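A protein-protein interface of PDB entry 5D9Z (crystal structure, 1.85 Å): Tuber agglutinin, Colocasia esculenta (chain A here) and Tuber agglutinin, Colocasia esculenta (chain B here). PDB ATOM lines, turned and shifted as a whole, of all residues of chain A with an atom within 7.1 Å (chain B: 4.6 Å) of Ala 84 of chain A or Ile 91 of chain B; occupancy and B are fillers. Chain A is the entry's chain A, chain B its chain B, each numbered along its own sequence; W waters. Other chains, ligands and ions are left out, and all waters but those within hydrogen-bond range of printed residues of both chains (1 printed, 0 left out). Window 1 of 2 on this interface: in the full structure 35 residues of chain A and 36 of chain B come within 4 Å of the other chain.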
ATOM      1  N   ASN A   4     -26.252  -1.637  14.037  1.00  0.00           N
ATOM      2  CA  ASN A   4     -27.394  -2.270  14.659  1.00  0.00           C
ATOM      3  C   ASN A   4     -27.088  -3.607  15.328  1.00  0.00           C
ATOM      4  O   ASN A   4     -28.010  -4.290  15.770  1.00  0.00           O
ATOM      5  CB  ASN A   4     -28.562  -2.389  13.680  1.00  0.00           C
ATOM      6  CG  ASN A   4     -28.139  -2.928  12.344  1.00  0.00           C
ATOM      7  OD1 ASN A   4     -27.070  -3.517  12.230  1.00  0.00           O
ATOM      8  ND2 ASN A   4     -28.975  -2.739  11.318  1.00  0.00           N
ATOM      9  N   TYR A   5     -25.810  -3.974  15.432  1.00  0.00           N
ATOM     10  CA  TYR A   5     -25.442  -5.172  16.186  1.00  0.00           C
ATOM     11  C   TYR A   5     -24.167  -5.072  16.967  1.00  0.00           C
ATOM     12  O   TYR A   5     -23.239  -4.321  16.643  1.00  0.00           O
ATOM     13  CB  TYR A   5     -25.301  -6.362  15.268  1.00  0.00           C
ATOM     14  CG  TYR A   5     -24.192  -6.185  14.280  1.00  0.00           C
ATOM     15  CD1 TYR A   5     -24.419  -5.561  13.067  1.00  0.00           C
ATOM     16  CD2 TYR A   5     -22.918  -6.642  14.557  1.00  0.00           C
ATOM     17  CE1 TYR A   5     -23.410  -5.400  12.163  1.00  0.00           C
ATOM     18  CE2 TYR A   5     -21.905  -6.484  13.662  1.00  0.00           C
ATOM     19  CZ  TYR A   5     -22.155  -5.863  12.468  1.00  0.00           C
ATOM     20  OH  TYR A   5     -21.131  -5.704  11.572  1.00  0.00           O
ATOM     21  N   LEU A   6     -24.116  -5.899  17.988  1.00  0.00           N
ATOM     22  CA  LEU A   6     -22.936  -6.017  18.770  1.00  0.00           C
ATOM     23  C   LEU A   6     -22.704  -7.495  18.781  1.00  0.00           C
ATOM     24  O   LEU A   6     -23.552  -8.252  19.279  1.00  0.00           O
ATOM     25  CB  LEU A   6     -23.205  -5.543  20.176  1.00  0.00           C
ATOM     26  CG  LEU A   6     -21.920  -5.422  20.955  1.00  0.00           C
ATOM     27  CD1 LEU A   6     -21.142  -4.279  20.359  1.00  0.00           C
ATOM     28  CD2 LEU A   6     -22.265  -5.159  22.382  1.00  0.00           C
ATOM     29  N   LEU A   7     -21.593  -7.905  18.173  1.00  0.00           N
ATOM     30  CA  LEU A   7     -21.201  -9.305  18.143  1.00  0.00           C
ATOM     31  C   LEU A   7     -20.611  -9.586  19.473  1.00  0.00           C
ATOM     32  O   LEU A   7     -20.155  -8.674  20.139  1.00  0.00           O
ATOM     33  CB  LEU A   7     -20.138  -9.561  17.094  1.00  0.00           C
ATOM     34  CG  LEU A   7     -20.611  -9.167  15.711  1.00  0.00           C
ATOM     35  CD1 LEU A   7     -19.637  -9.620  14.662  1.00  0.00           C
ATOM     36  CD2 LEU A   7     -21.959  -9.790  15.482  1.00  0.00           C
ATOM     37  N   SER A   8     -20.639 -10.848  19.868  1.00  0.00           N
ATOM     38  CA  SER A   8     -19.982 -11.274  21.091  1.00  0.00           C
ATOM     39  C   SER A   8     -18.505 -10.942  20.994  1.00  0.00           C
ATOM     40  O   SER A   8     -17.860 -11.193  19.974  1.00  0.00           O
ATOM     41  CB  SER A   8     -20.163 -12.767  21.297  1.00  0.00           C
ATOM     42  OG  SER A   8     -19.998 -13.449  20.069  1.00  0.00           O
ATOM     43  N   LEU A  55     -20.718  -8.566  25.136  1.00  0.00           N
ATOM     44  CA  LEU A  55     -21.515  -9.794  24.896  1.00  0.00           C
ATOM     45  C   LEU A  55     -20.600 -11.009  25.079  1.00  0.00           C
ATOM     46  O   LEU A  55     -19.512 -11.017  24.522  1.00  0.00           O
ATOM     47  CB  LEU A  55     -22.122  -9.805  23.480  1.00  0.00           C
ATOM     48  CG  LEU A  55     -23.087 -10.937  23.074  1.00  0.00           C
ATOM     49  CD1 LEU A  55     -24.329 -10.890  23.921  1.00  0.00           C
ATOM     50  CD2 LEU A  55     -23.484 -10.916  21.589  1.00  0.00           C
ATOM     51  N   GLY A  59     -23.442 -15.823  24.977  1.00  0.00           N
ATOM     52  CA  GLY A  59     -24.606 -15.039  24.603  1.00  0.00           C
ATOM     53  C   GLY A  59     -25.303 -14.347  25.761  1.00  0.00           C
ATOM     54  O   GLY A  59     -26.535 -14.339  25.851  1.00  0.00           O
ATOM     55  N   LEU A  61     -25.442 -10.552  27.842  1.00  0.00           N
ATOM     56  CA  LEU A  61     -25.053  -9.148  27.799  1.00  0.00           C
ATOM     57  C   LEU A  61     -24.647  -8.715  29.212  1.00  0.00           C
ATOM     58  O   LEU A  61     -25.371  -8.963  30.183  1.00  0.00           O
ATOM     59  CB  LEU A  61     -26.198  -8.290  27.261  1.00  0.00           C
ATOM     60  CG  LEU A  61     -26.593  -8.538  25.806  1.00  0.00           C
ATOM     61  CD1 LEU A  61     -28.022  -8.150  25.595  1.00  0.00           C
ATOM     62  CD2 LEU A  61     -25.710  -7.741  24.879  1.00  0.00           C
ATOM     63  N   ASN A  82     -20.416 -18.060  18.786  1.00  0.00           N
ATOM     64  CA  ASN A  82     -20.572 -16.649  18.432  1.00  0.00           C
ATOM     65  C   ASN A  82     -21.981 -16.128  18.629  1.00  0.00           C
ATOM     66  O   ASN A  82     -22.953 -16.839  18.404  1.00  0.00           O
ATOM     67  CB  ASN A  82     -20.154 -16.392  16.991  1.00  0.00           C
ATOM     68  CG  ASN A  82     -18.684 -16.603  16.781  1.00  0.00           C
ATOM     69  OD1 ASN A  82     -17.941 -16.793  17.747  1.00  0.00           O
ATOM     70  ND2 ASN A  82     -18.243 -16.564  15.517  1.00  0.00           N
ATOM     71  N   TYR A  83     -22.092 -14.873  19.041  1.00  0.00           N
ATOM     72  CA  TYR A  83     -23.402 -14.300  19.270  1.00  0.00           C
ATOM     73  C   TYR A  83     -23.488 -12.901  18.696  1.00  0.00           C
ATOM     74  O   TYR A  83     -22.468 -12.246  18.455  1.00  0.00           O
ATOM     75  CB  TYR A  83     -23.742 -14.314  20.756  1.00  0.00           C
ATOM     76  CG  TYR A  83     -24.042 -15.696  21.266  1.00  0.00           C
ATOM     77  CD1 TYR A  83     -23.027 -16.583  21.552  1.00  0.00           C
ATOM     78  CD2 TYR A  83     -25.340 -16.111  21.463  1.00  0.00           C
ATOM     79  CE1 TYR A  83     -23.295 -17.842  22.004  1.00  0.00           C
ATOM     80  CE2 TYR A  83     -25.617 -17.369  21.927  1.00  0.00           C
ATOM     81  CZ  TYR A  83     -24.589 -18.228  22.187  1.00  0.00           C
ATOM     82  OH  TYR A  83     -24.866 -19.483  22.643  1.00  0.00           O
ATOM     83  N   ALA A  84     -24.717 -12.473  18.436  1.00  0.00           N
ATOM     84  CA  ALA A  84     -24.984 -11.123  17.986  1.00  0.00           C
ATOM     85  C   ALA A  84     -26.117 -10.624  18.841  1.00  0.00           C
ATOM     86  O   ALA A  84     -27.117 -11.315  19.017  1.00  0.00           O
ATOM     87  CB  ALA A  84     -25.389 -11.117  16.543  1.00  0.00           C
ATOM     88  N   ALA A  85     -25.953  -9.444  19.414  1.00  0.00           N
ATOM     89  CA  ALA A  85     -27.090  -8.761  19.992  1.00  0.00           C
ATOM     90  C   ALA A  85     -27.532  -7.876  18.835  1.00  0.00           C
ATOM     91  O   ALA A  85     -26.669  -7.222  18.239  1.00  0.00           O
ATOM     92  CB  ALA A  85     -26.650  -7.938  21.164  1.00  0.00           C
ATOM     93  N   VAL A  86     -28.830  -7.878  18.483  1.00  0.00           N
ATOM     94  CA  VAL A  86     -29.355  -7.128  17.315  1.00  0.00           C
ATOM     95  C   VAL A  86     -30.549  -6.191  17.612  1.00  0.00           C
ATOM     96  O   VAL A  86     -31.449  -6.581  18.350  1.00  0.00           O
ATOM     97  CB  VAL A  86     -29.789  -8.085  16.198  1.00  0.00           C
ATOM     98  CG1 VAL A  86     -30.400  -7.308  15.048  1.00  0.00           C
ATOM     99  CG2 VAL A  86     -28.614  -8.902  15.714  1.00  0.00           C
ATOM    100  N   LEU A  93     -34.357  -5.426  21.598  1.00  0.00           N
ATOM    101  CA  LEU A  93     -32.960  -5.866  21.506  1.00  0.00           C
ATOM    102  C   LEU A  93     -32.939  -7.372  21.711  1.00  0.00           C
ATOM    103  O   LEU A  93     -33.368  -7.849  22.763  1.00  0.00           O
ATOM    104  CB  LEU A  93     -32.108  -5.199  22.584  1.00  0.00           C
ATOM    105  CG  LEU A  93     -30.607  -5.502  22.577  1.00  0.00           C
ATOM    106  CD1 LEU A  93     -30.098  -5.535  21.160  1.00  0.00           C
ATOM    107  CD2 LEU A  93     -29.858  -4.439  23.360  1.00  0.00           C
ATOM    108  N   VAL A  94     -32.461  -8.125  20.716  1.00  0.00           N
ATOM    109  CA  VAL A  94     -32.453  -9.581  20.797  1.00  0.00           C
ATOM    110  C   VAL A  94     -31.023 -10.146  20.721  1.00  0.00           C
ATOM    111  O   VAL A  94     -30.240  -9.726  19.856  1.00  0.00           O
ATOM    112  CB  VAL A  94     -33.321 -10.162  19.691  1.00  0.00           C
ATOM    113  CG1 VAL A  94     -33.412 -11.661  19.814  1.00  0.00           C
ATOM    114  CG2 VAL A  94     -34.704  -9.540  19.752  1.00  0.00           C
ATOM    115  N   VAL A  95     -30.672 -11.059  21.641  1.00  0.00           N
ATOM    116  CA  VAL A  95     -29.391 -11.777  21.578  1.00  0.00           C
ATOM    117  C   VAL A  95     -29.602 -13.062  20.808  1.00  0.00           C
ATOM    118  O   VAL A  95     -30.312 -13.959  21.252  1.00  0.00           O
ATOM    119  CB  VAL A  95     -28.812 -12.118  22.953  1.00  0.00           C
ATOM    120  CG1 VAL A  95     -27.634 -13.051  22.796  1.00  0.00           C
ATOM    121  CG2 VAL A  95     -28.368 -10.877  23.635  1.00  0.00           C
ATOM    122  N   PHE A  96     -29.012 -13.146  19.630  1.00  0.00           N
ATOM    123  CA  PHE A  96     -29.145 -14.353  18.841  1.00  0.00           C
ATOM    124  C   PHE A  96     -27.858 -15.114  18.980  1.00  0.00           C
ATOM    125  O   PHE A  96     -26.814 -14.521  19.267  1.00  0.00           O
ATOM    126  CB  PHE A  96     -29.298 -14.026  17.355  1.00  0.00           C
ATOM    127  CG  PHE A  96     -30.647 -13.460  16.961  1.00  0.00           C
ATOM    128  CD1 PHE A  96     -31.677 -14.297  16.564  1.00  0.00           C
ATOM    129  CD2 PHE A  96     -30.858 -12.085  16.926  1.00  0.00           C
ATOM    130  CE1 PHE A  96     -32.895 -13.781  16.179  1.00  0.00           C
ATOM    131  CE2 PHE A  96     -32.072 -11.558  16.537  1.00  0.00           C
ATOM    132  CZ  PHE A  96     -33.088 -12.406  16.162  1.00  0.00           C
ATOM    133  N   GLY A  97     -27.921 -16.418  18.726  1.00  0.00           N
ATOM    134  CA  GLY A  97     -26.729 -17.240  18.686  1.00  0.00           C
ATOM    135  C   GLY A  97     -26.921 -18.601  19.322  1.00  0.00           C
ATOM    136  O   GLY A  97     -27.901 -18.848  20.030  1.00  0.00           O
ATOM    137  N   PRO A  98     -25.949 -19.489  19.122  1.00  0.00           N
ATOM    138  CA  PRO A  98     -24.645 -19.254  18.497  1.00  0.00           C
ATOM    139  C   PRO A  98     -24.695 -19.228  16.979  1.00  0.00           C
ATOM    140  O   PRO A  98     -25.709 -19.615  16.416  1.00  0.00           O
ATOM    141  CB  PRO A  98     -23.851 -20.472  18.935  1.00  0.00           C
ATOM    142  CG  PRO A  98     -24.900 -21.554  18.969  1.00  0.00           C
ATOM    143  CD  PRO A  98     -26.108 -20.887  19.550  1.00  0.00           C
ATOM    144  N   SER A  99     -23.616 -18.775  16.340  1.00  0.00           N
ATOM    145  CA  SER A  99     -23.449 -18.880  14.889  1.00  0.00           C
ATOM    146  C   SER A  99     -23.851 -20.282  14.450  1.00  0.00           C
ATOM    147  O   SER A  99     -23.663 -21.225  15.200  1.00  0.00           O
ATOM    148  CB  SER A  99     -21.988 -18.593  14.517  1.00  0.00           C
ATOM    149  OG  SER A  99     -21.557 -19.342  13.395  1.00  0.00           O
ATOM    150  N   ASN B   7     -29.007  -4.959   6.150  1.00  0.00           N
ATOM    151  CA  ASN B   7     -27.962  -5.931   6.455  1.00  0.00           C
ATOM    152  C   ASN B   7     -28.453  -7.128   7.273  1.00  0.00           C
ATOM    153  O   ASN B   7     -27.655  -7.954   7.727  1.00  0.00           O
ATOM    154  CB  ASN B   7     -26.842  -5.252   7.215  1.00  0.00           C
ATOM    155  CG  ASN B   7     -27.297  -4.764   8.565  1.00  0.00           C
ATOM    156  OD1 ASN B   7     -28.481  -4.513   8.765  1.00  0.00           O
ATOM    157  ND2 ASN B   7     -26.369  -4.638   9.506  1.00  0.00           N
ATOM    158  N   LEU B   8     -29.760  -7.228   7.475  1.00  0.00           N
ATOM    159  CA  LEU B   8     -30.299  -8.327   8.257  1.00  0.00           C
ATOM    160  C   LEU B   8     -31.346  -9.051   7.461  1.00  0.00           C
ATOM    161  O   LEU B   8     -31.915  -8.494   6.536  1.00  0.00           O
ATOM    162  CB  LEU B   8     -30.944  -7.795   9.513  1.00  0.00           C
ATOM    163  CG  LEU B   8     -30.085  -6.774  10.218  1.00  0.00           C
ATOM    164  CD1 LEU B   8     -30.799  -6.243  11.431  1.00  0.00           C
ATOM    165  CD2 LEU B   8     -28.811  -7.452  10.620  1.00  0.00           C
ATOM    166  N   VAL B  89     -31.668 -15.093  12.467  1.00  0.00           N
ATOM    167  CA  VAL B  89     -31.335 -13.914  11.649  1.00  0.00           C
ATOM    168  C   VAL B  89     -30.106 -14.179  10.802  1.00  0.00           C
ATOM    169  O   VAL B  89     -29.269 -15.011  11.157  1.00  0.00           O
ATOM    170  CB  VAL B  89     -31.047 -12.667  12.496  1.00  0.00           C
ATOM    171  CG1 VAL B  89     -29.669 -12.755  13.092  1.00  0.00           C
ATOM    172  CG2 VAL B  89     -31.147 -11.416  11.636  1.00  0.00           C
ATOM    173  N   LEU B  90     -29.994 -13.479   9.682  1.00  0.00           N
ATOM    174  CA  LEU B  90     -28.811 -13.590   8.853  1.00  0.00           C
ATOM    175  C   LEU B  90     -28.229 -12.204   8.743  1.00  0.00           C
ATOM    176  O   LEU B  90     -28.854 -11.327   8.157  1.00  0.00           O
ATOM    177  CB  LEU B  90     -29.187 -14.093   7.469  1.00  0.00           C
ATOM    178  CG  LEU B  90     -28.200 -13.752   6.362  1.00  0.00           C
ATOM    179  CD1 LEU B  90     -26.885 -14.406   6.655  1.00  0.00           C
ATOM    180  CD2 LEU B  90     -28.756 -14.249   5.065  1.00  0.00           C
ATOM    181  N   ILE B  91     -27.052 -11.984   9.321  1.00  0.00           N
ATOM    182  CA  ILE B  91     -26.411 -10.681   9.211  1.00  0.00           C
ATOM    183  C   ILE B  91     -25.389 -10.725   8.095  1.00  0.00           C
ATOM    184  O   ILE B  91     -24.613 -11.671   8.031  1.00  0.00           O
ATOM    185  CB  ILE B  91     -25.704 -10.292  10.507  1.00  0.00           C
ATOM    186  CG1 ILE B  91     -26.651 -10.432  11.695  1.00  0.00           C
ATOM    187  CG2 ILE B  91     -25.162  -8.881  10.408  1.00  0.00           C
ATOM    188  CD1 ILE B  91     -26.030 -10.071  13.024  1.00  0.00           C
ATOM    189  N   LEU B  92     -25.404  -9.744   7.194  1.00  0.00           N
ATOM    190  CA  LEU B  92     -24.250  -9.491   6.320  1.00  0.00           C
ATOM    191  C   LEU B  92     -23.358  -8.540   7.110  1.00  0.00           C
ATOM    192  O   LEU B  92     -23.570  -7.330   7.066  1.00  0.00           O
ATOM    193  CB  LEU B  92     -24.659  -8.835   4.983  1.00  0.00           C
ATOM    194  CG  LEU B  92     -23.571  -8.558   3.940  1.00  0.00           C
ATOM    195  CD1 LEU B  92     -23.120  -9.864   3.366  1.00  0.00           C
ATOM    196  CD2 LEU B  92     -24.030  -7.634   2.819  1.00  0.00           C
ATOM    197  N   ARG B  93     -22.371  -9.064   7.842  1.00  0.00           N
ATOM    198  CA  ARG B  93     -21.570  -8.233   8.761  1.00  0.00           C
ATOM    199  C   ARG B  93     -20.630  -7.279   8.045  1.00  0.00           C
ATOM    200  O   ARG B  93     -20.239  -7.533   6.905  1.00  0.00           O
ATOM    201  CB  ARG B  93     -20.733  -9.098   9.699  1.00  0.00           C
ATOM    202  CG  ARG B  93     -21.448 -10.310  10.266  1.00  0.00           C
ATOM    203  CD  ARG B  93     -20.672 -10.950  11.444  1.00  0.00           C
ATOM    204  NE  ARG B  93     -19.225 -11.030  11.223  1.00  0.00           N
ATOM    205  CZ  ARG B  93     -18.423 -11.934  11.786  1.00  0.00           C
ATOM    206  NH1 ARG B  93     -18.923 -12.858  12.601  1.00  0.00           N
ATOM    207  NH2 ARG B  93     -17.121 -11.917  11.524  1.00  0.00           N
ATOM    208  N   PHE B  97     -18.451 -11.031   6.390  1.00  0.00           N
ATOM    209  CA  PHE B  97     -19.012 -12.346   6.603  1.00  0.00           C
ATOM    210  C   PHE B  97     -20.519 -12.279   6.576  1.00  0.00           C
ATOM    211  O   PHE B  97     -21.106 -11.416   7.221  1.00  0.00           O
ATOM    212  CB  PHE B  97     -18.572 -12.873   7.962  1.00  0.00           C
ATOM    213  CG  PHE B  97     -17.126 -13.302   8.013  1.00  0.00           C
ATOM    214  CD1 PHE B  97     -16.100 -12.367   7.946  1.00  0.00           C
ATOM    215  CD2 PHE B  97     -16.798 -14.655   8.138  1.00  0.00           C
ATOM    216  CE1 PHE B  97     -14.771 -12.778   7.985  1.00  0.00           C
ATOM    217  CE2 PHE B  97     -15.480 -15.075   8.182  1.00  0.00           C
ATOM    218  CZ  PHE B  97     -14.463 -14.137   8.105  1.00  0.00           C
ATOM    219  N   ALA B  98     -21.152 -13.174   5.827  1.00  0.00           N
ATOM    220  CA  ALA B  98     -22.581 -13.360   5.958  1.00  0.00           C
ATOM    221  C   ALA B  98     -22.639 -14.457   6.980  1.00  0.00           C
ATOM    222  O   ALA B  98     -22.034 -15.503   6.758  1.00  0.00           O
ATOM    223  N   VAL B  99     -23.283 -14.219   8.115  1.00  0.00           N
ATOM    224  CA  VAL B  99     -23.335 -15.232   9.170  1.00  0.00           C
ATOM    225  C   VAL B  99     -24.764 -15.381   9.662  1.00  0.00           C
ATOM    226  O   VAL B  99     -25.478 -14.388   9.800  1.00  0.00           O
ATOM    227  CB  VAL B  99     -22.417 -14.881  10.362  1.00  0.00           C
ATOM    228  CG1 VAL B  99     -22.508 -15.953  11.420  1.00  0.00           C
ATOM    229  CG2 VAL B  99     -20.984 -14.725   9.912  1.00  0.00           C
ATOM    230  N   TYR B 101     -26.963 -16.236  12.751  1.00  0.00           N
ATOM    231  CA  TYR B 101     -27.037 -16.459  14.196  1.00  0.00           C
ATOM    232  C   TYR B 101     -28.459 -16.873  14.615  1.00  0.00           C
ATOM    233  O   TYR B 101     -29.444 -16.458  13.996  1.00  0.00           O
ATOM    234  CB  TYR B 101     -26.628 -15.194  14.953  1.00  0.00           C
ATOM    235  CG  TYR B 101     -25.186 -14.742  14.757  1.00  0.00           C
ATOM    236  CD1 TYR B 101     -24.802 -14.033  13.630  1.00  0.00           C
ATOM    237  CD2 TYR B 101     -24.222 -14.987  15.730  1.00  0.00           C
ATOM    238  CE1 TYR B 101     -23.498 -13.597  13.472  1.00  0.00           C
ATOM    239  CE2 TYR B 101     -22.907 -14.555  15.576  1.00  0.00           C
ATOM    240  CZ  TYR B 101     -22.554 -13.866  14.446  1.00  0.00           C
ATOM    241  OH  TYR B 101     -21.252 -13.443  14.284  1.00  0.00           O
HETATM  242  O   HOH W   1     -17.625 -15.128  13.311  1.00  0.00           O
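Water W1 lies within hydrogen-bond range of the side-chain amide nitrogen (ND2) of Asn 82 of chain A (2.7 Å) and the guanidinium group (NH1) of Arg 93 of chain B (2.7 Å).
Among the printed residues, pairs that only touch across the chains: Asn 82 of chain A with Tyr 101 of chain B, Tyr 83 of chain A with Tyr 101 of chain B, Leu 7 of chain A with Arg 93 of chain B, Ala 84 of chain A with Tyr 101 of chain B, Ala 84 of chain A with Ile 91 of chain B, Phe 96 of chain A with Tyr 101 of chain B, Val 86 of chain A with Leu 8 of chain B, Tyr 5 of chain A with Arg 93 of chain B, Ser 99 of chain A with Tyr 101 of chain B, Leu 7 of chain A with Tyr 101 of chain B, Val 86 of chain A with Ile 91 of chain B and Asn 4 of chain A with Leu 8 of chain B.
Hydrophobic or aromatic side chains of chain B that line the printed part of chain A: Leu 8, Ile 91 and Tyr 101. Of the 20 printed residues of chain A, 9 touch a printed residue of chain B. Hydrophobic or aromatic side chains of chain A that line the printed part of chain B: Tyr 5, Leu 7, Ala 84, Val 86 and Phe 96. Among the printed residues, 13 pairs touch across the chains. Among the printed residues, no Asp or Glu carboxylate lies within 4 Å of a Lys or Arg side-chain nitrogen of the other chain.
O of Ile 91 of chain B lies within hydrogen-bond range of N of Val 99 of chain B (2.9 Å). The backbone carbonyl oxygen of Asn 7 of chain B sits at hydrogen-bond distance from the backbone NH of Leu 92 of chain B, at 2.9 Å. N of Val 86 of chain A is in hydrogen-bond range of O of Val 94 of chain A (2.7 Å). The backbone NH of Ser 8 of chain A lies within hydrogen-bond range of the backbone carbonyl oxygen of Tyr 83 of chain A (2.7 Å). N of Val 89 of chain B lies within hydrogen-bond range of O of Tyr 101 of chain B. The backbone carbonyl oxygen (O) of Ala 84 of chain A lies within hydrogen-bond range of the backbone NH (N) of Phe 96 of chain A (2.7 Å).
Printed residues of chain B within 4 Å of Ala 84 of chain A: Ile 91 (3.7 Å) and Tyr 101 (3.7 Å). Printed residues of chain A within 4 Å of Ile 91 of chain B: Ala 84 and Val 86. Printed residues of chain B within 4 Å of Tyr 83 of chain A: Tyr 101. Printed residues of chain B within 4 Å of Ser 99 of chain A: Tyr 101. Printed residues of chain A within 4 Å of Asn 7 of chain B: Asn 4 (3.0 Å). The nearest residue of chain A that does not touch Ile 91 of chain B is Tyr 5 of chain A (4.3 Å).
The side-chain amide nitrogen of Asn 7 of chain B sits at hydrogen-bond distance from the side-chain amide oxygen of Asn 4 of chain A, 3.0 Å away.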
